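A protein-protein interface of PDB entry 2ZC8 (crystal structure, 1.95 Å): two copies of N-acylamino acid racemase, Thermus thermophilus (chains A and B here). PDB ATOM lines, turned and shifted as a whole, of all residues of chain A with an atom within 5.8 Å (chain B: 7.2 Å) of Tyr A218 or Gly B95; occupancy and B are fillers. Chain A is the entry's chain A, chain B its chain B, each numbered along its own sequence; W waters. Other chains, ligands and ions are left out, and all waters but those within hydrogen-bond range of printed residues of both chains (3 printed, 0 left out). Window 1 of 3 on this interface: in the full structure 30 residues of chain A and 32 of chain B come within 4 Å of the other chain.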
ATOM      1  N   TYR A  55      -2.393  -4.801   6.636  1.00  0.00           N
ATOM      2  CA  TYR A  55      -2.328  -4.158   5.307  1.00  0.00           C
ATOM      3  C   TYR A  55      -3.248  -4.961   4.369  1.00  0.00           C
ATOM      4  O   TYR A  55      -4.046  -4.401   3.609  1.00  0.00           O
ATOM      5  CB  TYR A  55      -0.893  -4.193   4.774  1.00  0.00           C
ATOM      6  CG  TYR A  55      -0.800  -3.835   3.298  1.00  0.00           C
ATOM      7  CD1 TYR A  55      -0.816  -2.497   2.862  1.00  0.00           C
ATOM      8  CD2 TYR A  55      -0.696  -4.850   2.341  1.00  0.00           C
ATOM      9  CE1 TYR A  55      -0.719  -2.189   1.478  1.00  0.00           C
ATOM     10  CE2 TYR A  55      -0.610  -4.569   0.982  1.00  0.00           C
ATOM     11  CZ  TYR A  55      -0.619  -3.256   0.552  1.00  0.00           C
ATOM     12  OH  TYR A  55      -0.514  -3.043  -0.797  1.00  0.00           O
ATOM     13  N   ARG A  56      -3.105  -6.286   4.393  1.00  0.00           N
ATOM     14  CA  ARG A  56      -3.982  -7.150   3.608  1.00  0.00           C
ATOM     15  C   ARG A  56      -4.113  -8.513   4.317  1.00  0.00           C
ATOM     16  O   ARG A  56      -3.630  -8.677   5.435  1.00  0.00           O
ATOM     17  CB  ARG A  56      -3.534  -7.275   2.123  1.00  0.00           C
ATOM     18  CG  ARG A  56      -4.527  -6.517   1.160  1.00  0.00           C
ATOM     19  CD  ARG A  56      -4.305  -6.789  -0.351  1.00  0.00           C
ATOM     20  NE  ARG A  56      -5.368  -6.177  -1.186  1.00  0.00           N
ATOM     21  CZ  ARG A  56      -6.568  -6.730  -1.455  1.00  0.00           C
ATOM     22  NH1 ARG A  56      -6.919  -7.931  -0.987  1.00  0.00           N
ATOM     23  NH2 ARG A  56      -7.452  -6.055  -2.188  1.00  0.00           N
ATOM     24  N   GLU A  57      -4.760  -9.473   3.661  1.00  0.00           N
ATOM     25  CA  GLU A  57      -5.099 -10.758   4.261  1.00  0.00           C
ATOM     26  C   GLU A  57      -4.066 -11.825   4.609  1.00  0.00           C
ATOM     27  O   GLU A  57      -4.377 -12.745   5.383  1.00  0.00           O
ATOM     28  CB  GLU A  57      -6.188 -11.423   3.407  1.00  0.00           C
ATOM     29  CG  GLU A  57      -5.714 -11.943   2.061  1.00  0.00           C
ATOM     30  CD  GLU A  57      -5.394 -10.849   1.003  1.00  0.00           C
ATOM     31  OE1 GLU A  57      -4.632 -11.162   0.044  1.00  0.00           O
ATOM     32  OE2 GLU A  57      -5.896  -9.699   1.108  1.00  0.00           O
ATOM     33  N   SER A 191      -7.459   4.439   3.135  1.00  0.00           N
ATOM     34  CA  SER A 191      -8.799   3.838   3.151  1.00  0.00           C
ATOM     35  C   SER A 191      -9.620   4.376   4.323  1.00  0.00           C
ATOM     36  O   SER A 191     -10.485   3.682   4.871  1.00  0.00           O
ATOM     37  CB  SER A 191      -8.732   2.296   3.243  1.00  0.00           C
ATOM     38  OG  SER A 191      -8.022   1.709   2.159  1.00  0.00           O
ATOM     39  N   GLN A 214      -5.280   5.616  -2.341  1.00  0.00           N
ATOM     40  CA  GLN A 214      -6.276   4.692  -1.752  1.00  0.00           C
ATOM     41  C   GLN A 214      -7.203   5.283  -0.672  1.00  0.00           C
ATOM     42  O   GLN A 214      -7.208   4.838   0.477  1.00  0.00           O
ATOM     43  CB  GLN A 214      -5.500   3.480  -1.169  1.00  0.00           C
ATOM     44  CG  GLN A 214      -6.321   2.246  -0.879  1.00  0.00           C
ATOM     45  CD  GLN A 214      -6.683   1.439  -2.133  1.00  0.00           C
ATOM     46  OE1 GLN A 214      -5.856   1.244  -3.026  1.00  0.00           O
ATOM     47  NE2 GLN A 214      -7.916   0.947  -2.183  1.00  0.00           N
ATOM     48  N   LEU A 216     -10.582   5.143  -0.429  1.00  0.00           N
ATOM     49  CA  LEU A 216     -11.729   4.294  -0.088  1.00  0.00           C
ATOM     50  C   LEU A 216     -11.314   2.868   0.258  1.00  0.00           C
ATOM     51  O   LEU A 216     -10.121   2.607   0.518  1.00  0.00           O
ATOM     52  CB  LEU A 216     -12.784   4.336  -1.235  1.00  0.00           C
ATOM     53  CG  LEU A 216     -13.028   5.752  -1.785  1.00  0.00           C
ATOM     54  CD1 LEU A 216     -14.145   5.727  -2.883  1.00  0.00           C
ATOM     55  CD2 LEU A 216     -13.371   6.729  -0.625  1.00  0.00           C
ATOM     56  N   ALA A 217     -12.261   1.935   0.272  1.00  0.00           N
ATOM     57  CA  ALA A 217     -11.942   0.574   0.709  1.00  0.00           C
ATOM     58  C   ALA A 217     -10.741  -0.073   0.034  1.00  0.00           C
ATOM     59  O   ALA A 217     -10.526   0.051  -1.168  1.00  0.00           O
ATOM     60  CB  ALA A 217     -13.200  -0.364   0.594  1.00  0.00           C
ATOM     61  N   TYR A 218      -9.988  -0.834   0.829  1.00  0.00           N
ATOM     62  CA  TYR A 218      -8.774  -1.488   0.343  1.00  0.00           C
ATOM     63  C   TYR A 218      -8.970  -2.495  -0.797  1.00  0.00           C
ATOM     64  O   TYR A 218      -8.022  -2.779  -1.529  1.00  0.00           O
ATOM     65  CB  TYR A 218      -8.050  -2.170   1.522  1.00  0.00           C
ATOM     66  CG  TYR A 218      -8.582  -3.551   1.865  1.00  0.00           C
ATOM     67  CD1 TYR A 218      -7.964  -4.697   1.370  1.00  0.00           C
ATOM     68  CD2 TYR A 218      -9.714  -3.707   2.659  1.00  0.00           C
ATOM     69  CE1 TYR A 218      -8.468  -5.961   1.649  1.00  0.00           C
ATOM     70  CE2 TYR A 218     -10.218  -4.950   2.948  1.00  0.00           C
ATOM     71  CZ  TYR A 218      -9.595  -6.082   2.436  1.00  0.00           C
ATOM     72  OH  TYR A 218     -10.131  -7.324   2.678  1.00  0.00           O
ATOM     73  N   ASP A 219     -10.179  -3.033  -0.950  1.00  0.00           N
ATOM     74  CA  ASP A 219     -10.447  -4.014  -2.004  1.00  0.00           C
ATOM     75  C   ASP A 219     -11.486  -3.494  -2.996  1.00  0.00           C
ATOM     76  O   ASP A 219     -12.206  -4.292  -3.620  1.00  0.00           O
ATOM     77  CB  ASP A 219     -10.974  -5.327  -1.416  1.00  0.00           C
ATOM     78  CG  ASP A 219     -12.275  -5.130  -0.623  1.00  0.00           C
ATOM     79  OD1 ASP A 219     -12.585  -3.966  -0.225  1.00  0.00           O
ATOM     80  OD2 ASP A 219     -12.981  -6.140  -0.380  1.00  0.00           O
ATOM     81  N   ASP A 220     -11.567  -2.172  -3.118  1.00  0.00           N
ATOM     82  CA  ASP A 220     -12.535  -1.538  -4.011  1.00  0.00           C
ATOM     83  C   ASP A 220     -11.987  -0.915  -5.292  1.00  0.00           C
ATOM     84  O   ASP A 220     -10.913  -0.318  -5.282  1.00  0.00           O
ATOM     85  CB  ASP A 220     -13.286  -0.393  -3.290  1.00  0.00           C
ATOM     86  CG  ASP A 220     -14.114   0.449  -4.276  1.00  0.00           C
ATOM     87  OD1 ASP A 220     -15.308   0.123  -4.462  1.00  0.00           O
ATOM     88  OD2 ASP A 220     -13.555   1.404  -4.887  1.00  0.00           O
ATOM     89  N   HIS A 224     -14.079   3.872  -6.009  1.00  0.00           N
ATOM     90  CA  HIS A 224     -12.974   4.778  -6.370  1.00  0.00           C
ATOM     91  C   HIS A 224     -13.238   5.390  -7.753  1.00  0.00           C
ATOM     92  O   HIS A 224     -12.901   6.548  -8.003  1.00  0.00           O
ATOM     93  CB  HIS A 224     -11.640   4.026  -6.437  1.00  0.00           C
ATOM     94  CG  HIS A 224     -11.027   3.787  -5.095  1.00  0.00           C
ATOM     95  ND1 HIS A 224     -10.255   4.731  -4.444  1.00  0.00           N
ATOM     96  CD2 HIS A 224     -11.076   2.708  -4.280  1.00  0.00           C
ATOM     97  CE1 HIS A 224      -9.841   4.233  -3.289  1.00  0.00           C
ATOM     98  NE2 HIS A 224     -10.324   3.006  -3.168  1.00  0.00           N
ATOM     99  N   ASP A 238      -3.459   1.398  -4.490  1.00  0.00           N
ATOM    100  CA  ASP A 238      -2.421   0.588  -3.866  1.00  0.00           C
ATOM    101  C   ASP A 238      -3.045  -0.773  -3.541  1.00  0.00           C
ATOM    102  O   ASP A 238      -3.005  -1.677  -4.379  1.00  0.00           O
ATOM    103  CB  ASP A 238      -1.864   1.280  -2.590  1.00  0.00           C
ATOM    104  CG  ASP A 238      -0.906   0.368  -1.789  1.00  0.00           C
ATOM    105  OD1 ASP A 238      -0.681  -0.798  -2.177  1.00  0.00           O
ATOM    106  OD2 ASP A 238      -0.384   0.830  -0.774  1.00  0.00           O
ATOM    107  N   GLU A 239      -3.685  -0.904  -2.378  1.00  0.00           N
ATOM    108  CA  GLU A 239      -4.259  -2.193  -1.989  1.00  0.00           C
ATOM    109  C   GLU A 239      -5.222  -2.789  -2.995  1.00  0.00           C
ATOM    110  O   GLU A 239      -5.298  -4.003  -3.115  1.00  0.00           O
ATOM    111  CB  GLU A 239      -4.974  -2.104  -0.632  1.00  0.00           C
ATOM    112  CG  GLU A 239      -4.067  -1.910   0.565  1.00  0.00           C
ATOM    113  CD  GLU A 239      -3.851  -0.444   0.911  1.00  0.00           C
ATOM    114  OE1 GLU A 239      -3.781  -0.139   2.114  1.00  0.00           O
ATOM    115  OE2 GLU A 239      -3.753   0.390  -0.011  1.00  0.00           O
ATOM    116  N   SER A 240      -5.952  -1.957  -3.738  1.00  0.00           N
ATOM    117  CA  SER A 240      -6.917  -2.509  -4.706  1.00  0.00           C
ATOM    118  C   SER A 240      -6.281  -3.257  -5.882  1.00  0.00           C
ATOM    119  O   SER A 240      -6.931  -4.107  -6.498  1.00  0.00           O
ATOM    120  CB  SER A 240      -7.833  -1.396  -5.279  1.00  0.00           C
ATOM    121  OG  SER A 240      -8.631  -0.860  -4.243  1.00  0.00           O
ATOM    122  N   LEU A 241      -5.021  -2.958  -6.183  1.00  0.00           N
ATOM    123  CA  LEU A 241      -4.332  -3.589  -7.320  1.00  0.00           C
ATOM    124  C   LEU A 241      -3.644  -4.907  -6.974  1.00  0.00           C
ATOM    125  O   LEU A 241      -2.428  -4.952  -6.750  1.00  0.00           O
ATOM    126  CB  LEU A 241      -3.280  -2.639  -7.884  1.00  0.00           C
ATOM    127  CG  LEU A 241      -3.804  -1.398  -8.586  1.00  0.00           C
ATOM    128  CD1 LEU A 241      -2.589  -0.624  -9.099  1.00  0.00           C
ATOM    129  CD2 LEU A 241      -4.719  -1.788  -9.779  1.00  0.00           C
ATOM    130  N   GLU B  57      -8.734 -18.528  -1.180  1.00  0.00           N
ATOM    131  CA  GLU B  57      -7.398 -18.341  -0.653  1.00  0.00           C
ATOM    132  C   GLU B  57      -6.978 -18.832   0.714  1.00  0.00           C
ATOM    133  O   GLU B  57      -5.785 -18.887   0.993  1.00  0.00           O
ATOM    134  CB  GLU B  57      -7.045 -16.850  -0.761  1.00  0.00           C
ATOM    135  CG  GLU B  57      -7.845 -15.926   0.146  1.00  0.00           C
ATOM    136  CD  GLU B  57      -9.355 -15.781  -0.184  1.00  0.00           C
ATOM    137  OE1 GLU B  57      -9.796 -15.917  -1.364  1.00  0.00           O
ATOM    138  OE2 GLU B  57     -10.107 -15.468   0.771  1.00  0.00           O
ATOM    139  N   GLU B  58      -7.940 -19.183   1.557  1.00  0.00           N
ATOM    140  CA  GLU B  58      -7.609 -19.571   2.929  1.00  0.00           C
ATOM    141  C   GLU B  58      -7.233 -21.044   3.035  1.00  0.00           C
ATOM    142  O   GLU B  58      -7.605 -21.851   2.173  1.00  0.00           O
ATOM    143  CB  GLU B  58      -8.817 -19.280   3.842  1.00  0.00           C
ATOM    144  CG  GLU B  58      -9.229 -17.795   3.838  1.00  0.00           C
ATOM    145  CD  GLU B  58     -10.321 -17.465   4.829  1.00  0.00           C
ATOM    146  OE1 GLU B  58     -11.395 -17.017   4.372  1.00  0.00           O
ATOM    147  OE2 GLU B  58     -10.101 -17.631   6.061  1.00  0.00           O
ATOM    148  N   LEU B  66      -4.623 -17.741  12.727  1.00  0.00           N
ATOM    149  CA  LEU B  66      -5.444 -16.588  13.074  1.00  0.00           C
ATOM    150  C   LEU B  66      -6.342 -16.873  14.283  1.00  0.00           C
ATOM    151  O   LEU B  66      -6.413 -16.067  15.209  1.00  0.00           O
ATOM    152  CB  LEU B  66      -6.323 -16.158  11.878  1.00  0.00           C
ATOM    153  CG  LEU B  66      -5.538 -15.544  10.719  1.00  0.00           C
ATOM    154  CD1 LEU B  66      -6.501 -15.321   9.516  1.00  0.00           C
ATOM    155  CD2 LEU B  66      -4.921 -14.242  11.173  1.00  0.00           C
ATOM    156  N   PHE B  71      -7.350 -14.168  16.856  1.00  0.00           N
ATOM    157  CA  PHE B  71      -8.771 -13.948  17.191  1.00  0.00           C
ATOM    158  C   PHE B  71      -9.183 -14.363  18.617  1.00  0.00           C
ATOM    159  O   PHE B  71      -9.783 -13.588  19.352  1.00  0.00           O
ATOM    160  CB  PHE B  71      -9.682 -14.652  16.163  1.00  0.00           C
ATOM    161  CG  PHE B  71      -9.470 -14.201  14.722  1.00  0.00           C
ATOM    162  CD1 PHE B  71     -10.020 -14.945  13.668  1.00  0.00           C
ATOM    163  CD2 PHE B  71      -8.723 -13.058  14.422  1.00  0.00           C
ATOM    164  CE1 PHE B  71      -9.830 -14.556  12.300  1.00  0.00           C
ATOM    165  CE2 PHE B  71      -8.522 -12.649  13.054  1.00  0.00           C
ATOM    166  CZ  PHE B  71      -9.086 -13.413  11.999  1.00  0.00           C
ATOM    167  N   LEU B  90     -13.116  -8.097  15.590  1.00  0.00           N
ATOM    168  CA  LEU B  90     -12.258  -8.656  14.530  1.00  0.00           C
ATOM    169  C   LEU B  90     -12.088  -7.757  13.320  1.00  0.00           C
ATOM    170  O   LEU B  90     -11.403  -8.138  12.368  1.00  0.00           O
ATOM    171  CB  LEU B  90     -12.823  -9.985  14.043  1.00  0.00           C
ATOM    172  CG  LEU B  90     -13.087 -10.978  15.177  1.00  0.00           C
ATOM    173  CD1 LEU B  90     -13.650 -12.266  14.587  1.00  0.00           C
ATOM    174  CD2 LEU B  90     -11.779 -11.228  15.951  1.00  0.00           C
ATOM    175  N   ALA B  91     -12.694  -6.575  13.370  1.00  0.00           N
ATOM    176  CA  ALA B  91     -12.672  -5.649  12.242  1.00  0.00           C
ATOM    177  C   ALA B  91     -11.298  -5.226  11.733  1.00  0.00           C
ATOM    178  O   ALA B  91     -11.098  -5.075  10.528  1.00  0.00           O
ATOM    179  CB  ALA B  91     -13.520  -4.414  12.575  1.00  0.00           C
ATOM    180  N   PRO B  92     -10.332  -5.030  12.637  1.00  0.00           N
ATOM    181  CA  PRO B  92      -9.001  -4.619  12.183  1.00  0.00           C
ATOM    182  C   PRO B  92      -8.293  -5.626  11.239  1.00  0.00           C
ATOM    183  O   PRO B  92      -7.362  -5.258  10.507  1.00  0.00           O
ATOM    184  CB  PRO B  92      -8.236  -4.444  13.493  1.00  0.00           C
ATOM    185  CG  PRO B  92      -9.315  -4.072  14.479  1.00  0.00           C
ATOM    186  CD  PRO B  92     -10.407  -5.040  14.113  1.00  0.00           C
ATOM    187  N   PHE B  93      -8.726  -6.885  11.264  1.00  0.00           N
ATOM    188  CA  PHE B  93      -8.064  -7.915  10.464  1.00  0.00           C
ATOM    189  C   PHE B  93      -8.713  -8.026   9.101  1.00  0.00           C
ATOM    190  O   PHE B  93      -9.909  -8.275   9.005  1.00  0.00           O
ATOM    191  CB  PHE B  93      -8.094  -9.235  11.257  1.00  0.00           C
ATOM    192  CG  PHE B  93      -7.586  -9.064  12.661  1.00  0.00           C
ATOM    193  CD1 PHE B  93      -8.449  -9.171  13.754  1.00  0.00           C
ATOM    194  CD2 PHE B  93      -6.268  -8.654  12.881  1.00  0.00           C
ATOM    195  CE1 PHE B  93      -8.010  -8.857  15.041  1.00  0.00           C
ATOM    196  CE2 PHE B  93      -5.818  -8.335  14.174  1.00  0.00           C
ATOM    197  CZ  PHE B  93      -6.702  -8.438  15.254  1.00  0.00           C
ATOM    198  N   ARG B  94      -7.925  -7.818   8.047  1.00  0.00           N
ATOM    199  CA  ARG B  94      -8.482  -7.841   6.700  1.00  0.00           C
ATOM    200  C   ARG B  94      -8.689  -9.231   6.121  1.00  0.00           C
ATOM    201  O   ARG B  94      -7.896 -10.145   6.362  1.00  0.00           O
ATOM    202  CB  ARG B  94      -7.603  -6.977   5.753  1.00  0.00           C
ATOM    203  CG  ARG B  94      -7.716  -5.468   6.045  1.00  0.00           C
ATOM    204  CD  ARG B  94      -6.910  -4.527   5.124  1.00  0.00           C
ATOM    205  NE  ARG B  94      -7.265  -3.119   5.387  1.00  0.00           N
ATOM    206  CZ  ARG B  94      -6.595  -2.066   4.916  1.00  0.00           C
ATOM    207  NH1 ARG B  94      -5.506  -2.230   4.148  1.00  0.00           N
ATOM    208  NH2 ARG B  94      -7.018  -0.836   5.203  1.00  0.00           N
ATOM    209  N   GLY B  95      -9.772  -9.381   5.358  1.00  0.00           N
ATOM    210  CA  GLY B  95     -10.084 -10.658   4.719  1.00  0.00           C
ATOM    211  C   GLY B  95     -10.271 -11.809   5.691  1.00  0.00           C
ATOM    212  O   GLY B  95     -10.805 -11.630   6.789  1.00  0.00           O
ATOM    213  N   ASN B  96      -9.850 -12.998   5.268  1.00  0.00           N
ATOM    214  CA  ASN B  96      -9.946 -14.196   6.107  1.00  0.00           C
ATOM    215  C   ASN B  96     -11.340 -14.430   6.663  1.00  0.00           C
ATOM    216  O   ASN B  96     -11.489 -14.748   7.839  1.00  0.00           O
ATOM    217  CB  ASN B  96      -8.913 -14.092   7.246  1.00  0.00           C
ATOM    218  CG  ASN B  96      -7.515 -14.038   6.707  1.00  0.00           C
ATOM    219  OD1 ASN B  96      -6.985 -15.049   6.279  1.00  0.00           O
ATOM    220  ND2 ASN B  96      -6.931 -12.840   6.664  1.00  0.00           N
ATOM    221  N   PRO B  97     -12.377 -14.334   5.805  1.00  0.00           N
ATOM    222  CA  PRO B  97     -13.750 -14.541   6.271  1.00  0.00           C
ATOM    223  C   PRO B  97     -14.065 -15.936   6.822  1.00  0.00           C
ATOM    224  O   PRO B  97     -14.835 -16.048   7.765  1.00  0.00           O
ATOM    225  CB  PRO B  97     -14.604 -14.210   5.020  1.00  0.00           C
ATOM    226  CG  PRO B  97     -13.690 -14.596   3.888  1.00  0.00           C
ATOM    227  CD  PRO B  97     -12.370 -13.969   4.363  1.00  0.00           C
ATOM    228  N   MET B  98     -13.476 -16.986   6.236  1.00  0.00           N
ATOM    229  CA  MET B  98     -13.758 -18.352   6.695  1.00  0.00           C
ATOM    230  C   MET B  98     -13.145 -18.564   8.082  1.00  0.00           C
ATOM    231  O   MET B  98     -13.766 -19.208   8.934  1.00  0.00           O
ATOM    232  CB  MET B  98     -13.218 -19.394   5.704  1.00  0.00           C
ATOM    233  CG  MET B  98     -13.834 -19.309   4.315  1.00  0.00           C
ATOM    234  SD  MET B  98     -13.159 -20.595   3.225  1.00  0.00           S
ATOM    235  CE  MET B  98     -14.197 -20.382   1.804  1.00  0.00           C
ATOM    236  N   ALA B  99     -11.948 -18.011   8.309  1.00  0.00           N
ATOM    237  CA  ALA B  99     -11.318 -18.131   9.632  1.00  0.00           C
ATOM    238  C   ALA B  99     -12.183 -17.348  10.632  1.00  0.00           C
ATOM    239  O   ALA B  99     -12.469 -17.834  11.732  1.00  0.00           O
ATOM    240  CB  ALA B  99      -9.882 -17.569   9.623  1.00  0.00           C
ATOM    241  N   LYS B 100     -12.592 -16.127  10.276  1.00  0.00           N
ATOM    242  CA  LYS B 100     -13.453 -15.360  11.197  1.00  0.00           C
ATOM    243  C   LYS B 100     -14.777 -16.086  11.451  1.00  0.00           C
ATOM    244  O   LYS B 100     -15.308 -16.061  12.576  1.00  0.00           O
ATOM    245  CB  LYS B 100     -13.787 -13.965  10.631  1.00  0.00           C
ATOM    246  CG  LYS B 100     -12.603 -12.982  10.594  1.00  0.00           C
ATOM    247  CD  LYS B 100     -13.106 -11.538  10.248  1.00  0.00           C
ATOM    248  CE  LYS B 100     -11.919 -10.574  10.173  1.00  0.00           C
ATOM    249  NZ  LYS B 100     -12.298  -9.145   9.874  1.00  0.00           N
ATOM    250  N   GLU B 245     -20.491  -5.835   0.969  1.00  0.00           N
ATOM    251  CA  GLU B 245     -20.086  -4.819  -0.006  1.00  0.00           C
ATOM    252  C   GLU B 245     -20.050  -5.393  -1.424  1.00  0.00           C
ATOM    253  O   GLU B 245     -20.465  -4.740  -2.373  1.00  0.00           O
ATOM    254  CB  GLU B 245     -18.713  -4.240   0.337  1.00  0.00           C
ATOM    255  CG  GLU B 245     -18.693  -3.470   1.635  1.00  0.00           C
ATOM    256  CD  GLU B 245     -17.277  -3.092   2.032  1.00  0.00           C
ATOM    257  OE1 GLU B 245     -16.505  -4.001   2.405  1.00  0.00           O
ATOM    258  OE2 GLU B 245     -16.935  -1.894   1.957  1.00  0.00           O
HETATM  259  O   HOH W   1     -13.822  -4.010   2.263  1.00  0.00           O
HETATM  260  O   HOH W   2      -4.326 -15.279   6.320  1.00  0.00           O
HETATM  261  O   HOH W   3     -15.651  -5.770  -0.467  1.00  0.00           O
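The backbone carbonyl oxygen (O) of Glu A57 is in hydrogen-bond range of the side-chain amide nitrogen (ND2) of Asn B96.
The backbone NH of Gly B95 sits at hydrogen-bond distance from the side-chain hydroxyl of Tyr A218 (3.4 Å).
NH1 of Arg B94 lies within salt-bridge range of OE1 of Glu A239, at 3.4 Å.
O of Tyr A55 is in hydrogen-bond range of NH1 of Arg B94 (2.7 Å).
N of Tyr A218 is in hydrogen-bond range of OG of Ser A191 (3.5 Å).
O of Arg B94 sits at hydrogen-bond distance from ND2 of Asn B96, at 2.9 Å.
The backbone NH of Ser A240 is in hydrogen-bond range of the backbone carbonyl oxygen of Tyr A218, 3.1 Å away.
O of Tyr A218 is in hydrogen-bond range of NH2 of Arg A56.
NH1 of Arg A56 is in salt-bridge range of OE2 of Glu A57 (2.9 Å).
The guanidinium group (NE) of Arg A56 lies within hydrogen-bond range of the backbone carbonyl oxygen (O) of Glu A239.
Arg B94 touches Glu A57 (O to CA, 3.6 Å).
Arg B94 touches Tyr A218 (NH1 to CB, 3.7 Å).
Of the printed residues of chain B, Tyr A55 touches Arg B94.
Of the printed residues of chain B, Glu A57 touches Arg B94 (3.6 Å) and Asn B96 (2.9 Å).
Tyr A218 touches just these residues of chain B: Arg B94 (3.7 Å) and Gly B95 (3.4 Å).
Asp A238 touches none of the printed residues of chain B.
Of the printed residues of chain B, Glu A239 touches Arg B94.
Of the printed residues of chain A, Arg B94 touches Tyr A55 (2.7 Å), Glu A57 (3.6 Å), Tyr A218 (3.7 Å) and Glu A239 (3.4 Å).
Printed residues of chain A within 4 Å of Asn B96: Glu A57.
The nearest residue of chain B that does not touch Tyr A218 is Asn B96 (6.2 Å).
Of the 16 printed residues of chain B, 3 touch a printed residue of chain A.
Of the 15 printed residues of chain A, 4 touch a printed residue of chain B.
Along chain A the printed residues that touch a printed residue of chain B span positions 55 to 239.
Among the printed residues, 6 pairs touch across the chains.
Among the printed residues, Asp or Glu carboxylates within 4 Å of a Lys or Arg side-chain nitrogen of the other chain: Glu A239 with Arg B94.
1 position is printed for both chains.
Of the 6 pairs that touch across the chains among the printed residues, none has its exchanged pair printed and touching as well.
Water W2 lies within hydrogen-bond range of the side-chain amide oxygen (OD1) of Asn B96 and the backbone carbonyl oxygen (O) of Glu A57.
Water W1 lies within hydrogen-bond range of OE1 of Glu B245 and OD1 of Asp A219.
Water W3 bridges the side-chain carboxylate (OD2) of Asp A219 (2.7 Å) and the side-chain carboxylate (OE1) of Glu B245 (3.5 Å).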
